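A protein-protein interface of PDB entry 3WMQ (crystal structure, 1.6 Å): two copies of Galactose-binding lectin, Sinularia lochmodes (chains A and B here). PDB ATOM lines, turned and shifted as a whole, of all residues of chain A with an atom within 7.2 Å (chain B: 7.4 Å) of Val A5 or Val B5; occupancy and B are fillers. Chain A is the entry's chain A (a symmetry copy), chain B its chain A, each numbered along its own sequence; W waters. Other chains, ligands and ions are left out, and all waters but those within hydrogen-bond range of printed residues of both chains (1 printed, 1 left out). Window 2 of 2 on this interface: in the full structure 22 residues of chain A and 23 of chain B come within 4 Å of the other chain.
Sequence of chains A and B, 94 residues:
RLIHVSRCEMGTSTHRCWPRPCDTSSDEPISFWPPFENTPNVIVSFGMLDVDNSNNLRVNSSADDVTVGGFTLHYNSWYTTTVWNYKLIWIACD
O of Ser A6 is in hydrogen-bond range of N of Ser B6, 2.9 Å away.
OG of Ser B6 is in hydrogen-bond range of N of Cys A8.
The side-chain hydroxyl (OG) of Ser B6 is in hydrogen-bond range of the chain-end carboxylate (O) of Asp B94 (2.8 Å).
The side-chain carboxylate (OD1) of Asp B94 is in hydrogen-bond range of the backbone NH (N) of Arg B7.
The chain-end carboxylate of Asp A94 lies within hydrogen-bond range of the side-chain hydroxyl of Ser A6 (2.8 Å).
N of Arg A7 is in hydrogen-bond range of OD1 of Asp A94 (2.9 Å).
Among the printed residues, pairs that only touch across the chains: Val A5 with Val B5 (3.7 Å), Ser A6 with Val B5 (3.6 Å), Arg A7 with His B4 (3.4 Å), Arg A7 with Ser B6 (3.7 Å) and Cys A8 with Asp B94 (3.9 Å).
Val A5 touches just one residue of chain B: Val B5 (3.7 Å).
Val B5 touches two residues of chain A.
Of the printed residues of chain B, Ser A6 touches Val B5 and Ser B6.
Of the printed residues of chain A, Asp B94 touches Cys A8.
Of the printed residues of chain B, Arg A7 touches His B4 (3.4 Å) and Ser B6 (3.7 Å).
Of the printed residues of chain B, Cys A8 touches Ser B6 (2.8 Å) and Asp B94 (3.9 Å).
Ile B3 touches none of the printed residues of chain A.
The nearest residue of chain B that does not touch Val A5 is Ile B3 (5.3 Å).
The nearest residue of chain A that does not touch Val B5 is Arg A7 (4.3 Å).
The nearest printed residue of chain A that does not touch His B4 is Ser A6 (4.6 Å).
Hydrophobic or aromatic side chains of chain B within 4 Å of the printed part of chain A: His B4 and Val B5.
Hydrophobic or aromatic side chains of chain A within 4 Å of the printed part of chain B: Val A5.
Val B5 touches its own counterpart, Val A5.
Ser A6 touches its own counterpart, Ser B6.
Arg A7 touches His B4, but with the chains exchanged His A4 does not touch Arg B7 (10.1 Å).
Arg A7 touches Ser B6, but with the chains exchanged Ser A6 does not touch Arg B7 (5.6 Å).
Water W1 bridges O of Cys A8 and O of Asp B94.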
ATOM      1  N   ILE A   3       6.957  -7.586 -24.224  1.00  0.00           N
ATOM      2  CA  ILE A   3       6.660  -8.054 -25.572  1.00  0.00           C
ATOM      3  C   ILE A   3       5.257  -8.627 -25.613  1.00  0.00           C
ATOM      4  O   ILE A   3       4.675  -8.958 -24.580  1.00  0.00           O
ATOM      5  CB  ILE A   3       7.647  -9.145 -26.084  1.00  0.00           C
ATOM      6  CG1 ILE A   3       7.493 -10.436 -25.282  1.00  0.00           C
ATOM      7  CG2 ILE A   3       9.071  -8.634 -26.030  1.00  0.00           C
ATOM      8  CD1 ILE A   3       8.235 -11.612 -25.890  1.00  0.00           C
ATOM      9  N   HIS A   4       4.713  -8.727 -26.819  1.00  0.00           N
ATOM     10  CA  HIS A   4       3.377  -9.264 -27.014  1.00  0.00           C
ATOM     11  C   HIS A   4       3.488 -10.645 -27.638  1.00  0.00           C
ATOM     12  O   HIS A   4       4.017 -10.784 -28.737  1.00  0.00           O
ATOM     13  CB  HIS A   4       2.571  -8.368 -27.963  1.00  0.00           C
ATOM     14  CG  HIS A   4       2.270  -7.007 -27.416  1.00  0.00           C
ATOM     15  ND1 HIS A   4       1.145  -6.735 -26.668  1.00  0.00           N
ATOM     16  CD2 HIS A   4       2.956  -5.842 -27.503  1.00  0.00           C
ATOM     17  CE1 HIS A   4       1.150  -5.461 -26.317  1.00  0.00           C
ATOM     18  NE2 HIS A   4       2.238  -4.898 -26.810  1.00  0.00           N
ATOM     19  N   VAL A   5       3.013 -11.667 -26.938  1.00  0.00           N
ATOM     20  CA  VAL A   5       3.035 -13.011 -27.497  1.00  0.00           C
ATOM     21  C   VAL A   5       1.729 -13.683 -27.180  1.00  0.00           C
ATOM     22  O   VAL A   5       1.044 -13.327 -26.219  1.00  0.00           O
ATOM     23  CB  VAL A   5       4.181 -13.904 -26.961  1.00  0.00           C
ATOM     24  CG1 VAL A   5       5.523 -13.289 -27.291  1.00  0.00           C
ATOM     25  CG2 VAL A   5       4.015 -14.148 -25.477  1.00  0.00           C
ATOM     26  N   SER A   6       1.389 -14.667 -27.995  1.00  0.00           N
ATOM     27  CA  SER A   6       0.142 -15.371 -27.814  1.00  0.00           C
ATOM     28  C   SER A   6       0.315 -16.861 -27.662  1.00  0.00           C
ATOM     29  O   SER A   6       1.237 -17.452 -28.209  1.00  0.00           O
ATOM     30  CB  SER A   6      -0.778 -15.158 -29.024  1.00  0.00           C
ATOM     31  OG  SER A   6      -1.062 -13.800 -29.262  1.00  0.00           O
ATOM     32  N   ARG A   7      -0.596 -17.461 -26.912  1.00  0.00           N
ATOM     33  CA  ARG A   7      -0.628 -18.901 -26.774  1.00  0.00           C
ATOM     34  C   ARG A   7      -1.866 -19.145 -27.591  1.00  0.00           C
ATOM     35  O   ARG A   7      -2.858 -18.447 -27.401  1.00  0.00           O
ATOM     36  CB  ARG A   7      -0.901 -19.372 -25.344  1.00  0.00           C
ATOM     37  CG  ARG A   7      -1.392 -20.835 -25.314  1.00  0.00           C
ATOM     38  CD  ARG A   7      -1.844 -21.226 -23.925  1.00  0.00           C
ATOM     39  NE  ARG A   7      -2.421 -22.565 -23.857  1.00  0.00           N
ATOM     40  CZ  ARG A   7      -2.962 -23.076 -22.756  1.00  0.00           C
ATOM     41  NH1 ARG A   7      -2.996 -22.358 -21.641  1.00  0.00           N
ATOM     42  NH2 ARG A   7      -3.471 -24.301 -22.767  1.00  0.00           N
ATOM     43  N   CYS A   8      -1.808 -20.097 -28.509  1.00  0.00           N
ATOM     44  CA  CYS A   8      -2.982 -20.406 -29.315  1.00  0.00           C
ATOM     45  C   CYS A   8      -3.291 -21.894 -29.229  1.00  0.00           C
ATOM     46  O   CYS A   8      -2.388 -22.727 -29.254  1.00  0.00           O
ATOM     47  CB  CYS A   8      -2.768 -20.057 -30.791  1.00  0.00           C
ATOM     48  SG  CYS A   8      -2.615 -18.320 -31.316  1.00  0.00           S
ATOM     49  N   ASP A  94      -4.577 -15.803 -26.751  1.00  0.00           N
ATOM     50  CA  ASP A  94      -4.635 -14.703 -25.803  1.00  0.00           C
ATOM     51  C   ASP A  94      -3.580 -13.692 -26.223  1.00  0.00           C
ATOM     52  O   ASP A  94      -3.182 -13.756 -27.411  1.00  0.00           O
ATOM     53  CB  ASP A  94      -4.429 -15.192 -24.350  1.00  0.00           C
ATOM     54  CG  ASP A  94      -3.034 -15.729 -24.083  1.00  0.00           C
ATOM     55  OD1 ASP A  94      -2.286 -15.984 -25.047  1.00  0.00           O
ATOM     56  OD2 ASP A  94      -2.697 -15.907 -22.891  1.00  0.00           O
ATOM     57  OXT ASP A  94      -3.195 -12.850 -25.385  1.00  0.00           O
ATOM     58  N   ILE B   3       6.232 -21.026 -19.646  1.00  0.00           N
ATOM     59  CA  ILE B   3       5.123 -20.295 -20.244  1.00  0.00           C
ATOM     60  C   ILE B   3       4.674 -21.000 -21.509  1.00  0.00           C
ATOM     61  O   ILE B   3       5.405 -21.813 -22.076  1.00  0.00           O
ATOM     62  CB  ILE B   3       5.470 -18.820 -20.604  1.00  0.00           C
ATOM     63  CG1 ILE B   3       6.501 -18.764 -21.729  1.00  0.00           C
ATOM     64  CG2 ILE B   3       5.958 -18.079 -19.377  1.00  0.00           C
ATOM     65  CD1 ILE B   3       6.691 -17.372 -22.301  1.00  0.00           C
ATOM     66  N   HIS B   4       3.458 -20.689 -21.940  1.00  0.00           N
ATOM     67  CA  HIS B   4       2.898 -21.281 -23.142  1.00  0.00           C
ATOM     68  C   HIS B   4       2.870 -20.230 -24.240  1.00  0.00           C
ATOM     69  O   HIS B   4       2.216 -19.202 -24.093  1.00  0.00           O
ATOM     70  CB  HIS B   4       1.460 -21.753 -22.890  1.00  0.00           C
ATOM     71  CG  HIS B   4       1.348 -22.887 -21.919  1.00  0.00           C
ATOM     72  ND1 HIS B   4       1.408 -24.208 -22.304  1.00  0.00           N
ATOM     73  CD2 HIS B   4       1.188 -22.893 -20.573  1.00  0.00           C
ATOM     74  CE1 HIS B   4       1.290 -24.981 -21.239  1.00  0.00           C
ATOM     75  NE2 HIS B   4       1.156 -24.208 -20.177  1.00  0.00           N
ATOM     76  N   VAL B   5       3.592 -20.469 -25.328  1.00  0.00           N
ATOM     77  CA  VAL B   5       3.568 -19.534 -26.442  1.00  0.00           C
ATOM     78  C   VAL B   5       3.497 -20.317 -27.724  1.00  0.00           C
ATOM     79  O   VAL B   5       3.898 -21.481 -27.784  1.00  0.00           O
ATOM     80  CB  VAL B   5       4.802 -18.600 -26.515  1.00  0.00           C
ATOM     81  CG1 VAL B   5       4.898 -17.760 -25.261  1.00  0.00           C
ATOM     82  CG2 VAL B   5       6.062 -19.403 -26.760  1.00  0.00           C
ATOM     83  N   SER B   6       2.986 -19.664 -28.754  1.00  0.00           N
ATOM     84  CA  SER B   6       2.835 -20.318 -30.033  1.00  0.00           C
ATOM     85  C   SER B   6       3.524 -19.590 -31.159  1.00  0.00           C
ATOM     86  O   SER B   6       3.651 -18.372 -31.145  1.00  0.00           O
ATOM     87  CB  SER B   6       1.352 -20.415 -30.416  1.00  0.00           C
ATOM     88  OG  SER B   6       0.586 -21.115 -29.465  1.00  0.00           O
ATOM     89  N   ARG B   7       3.962 -20.359 -32.143  1.00  0.00           N
ATOM     90  CA  ARG B   7       4.535 -19.792 -33.344  1.00  0.00           C
ATOM     91  C   ARG B   7       3.397 -20.115 -34.272  1.00  0.00           C
ATOM     92  O   ARG B   7       2.904 -21.239 -34.249  1.00  0.00           O
ATOM     93  CB  ARG B   7       5.777 -20.536 -33.839  1.00  0.00           C
ATOM     94  CG  ARG B   7       6.071 -20.224 -35.322  1.00  0.00           C
ATOM     95  CD  ARG B   7       7.175 -21.109 -35.853  1.00  0.00           C
ATOM     96  NE  ARG B   7       7.423 -20.936 -37.281  1.00  0.00           N
ATOM     97  CZ  ARG B   7       8.287 -21.673 -37.972  1.00  0.00           C
ATOM     98  NH1 ARG B   7       8.977 -22.628 -37.361  1.00  0.00           N
ATOM     99  NH2 ARG B   7       8.460 -21.462 -39.269  1.00  0.00           N
ATOM    100  N   ASN B  38       7.941 -28.023 -32.526  1.00  0.00           N
ATOM    101  CA  ASN B  38       7.057 -29.171 -32.253  1.00  0.00           C
ATOM    102  C   ASN B  38       6.073 -29.155 -33.394  1.00  0.00           C
ATOM    103  O   ASN B  38       5.818 -28.110 -34.000  1.00  0.00           O
ATOM    104  CB  ASN B  38       6.246 -29.109 -30.939  1.00  0.00           C
ATOM    105  CG  ASN B  38       7.103 -29.005 -29.710  1.00  0.00           C
ATOM    106  OD1 ASN B  38       7.935 -29.867 -29.415  1.00  0.00           O
ATOM    107  ND2 ASN B  38       6.864 -27.960 -28.948  1.00  0.00           N
ATOM    108  N   CYS B  93      -0.302 -23.506 -35.828  1.00  0.00           N
ATOM    109  CA  CYS B  93       0.362 -22.994 -34.634  1.00  0.00           C
ATOM    110  C   CYS B  93       0.755 -24.166 -33.750  1.00  0.00           C
ATOM    111  O   CYS B  93       0.074 -25.190 -33.729  1.00  0.00           O
ATOM    112  CB  CYS B  93      -0.551 -22.075 -33.816  1.00  0.00           C
ATOM    113  SG  CYS B  93      -1.422 -20.677 -34.606  1.00  0.00           S
ATOM    114  N   ASP B  94       1.852 -24.021 -33.016  1.00  0.00           N
ATOM    115  CA  ASP B  94       2.267 -25.079 -32.110  1.00  0.00           C
ATOM    116  C   ASP B  94       2.035 -24.575 -30.694  1.00  0.00           C
ATOM    117  O   ASP B  94       1.225 -23.626 -30.563  1.00  0.00           O
ATOM    118  CB  ASP B  94       3.739 -25.489 -32.348  1.00  0.00           C
ATOM    119  CG  ASP B  94       4.737 -24.399 -31.995  1.00  0.00           C
ATOM    120  OD1 ASP B  94       4.328 -23.236 -31.815  1.00  0.00           O
ATOM    121  OD2 ASP B  94       5.944 -24.721 -31.913  1.00  0.00           O
ATOM    122  OXT ASP B  94       2.630 -25.141 -29.755  1.00  0.00           O
HETATM  123  O   HOH W   1      -0.302 -24.305 -28.110  1.00  0.00           O
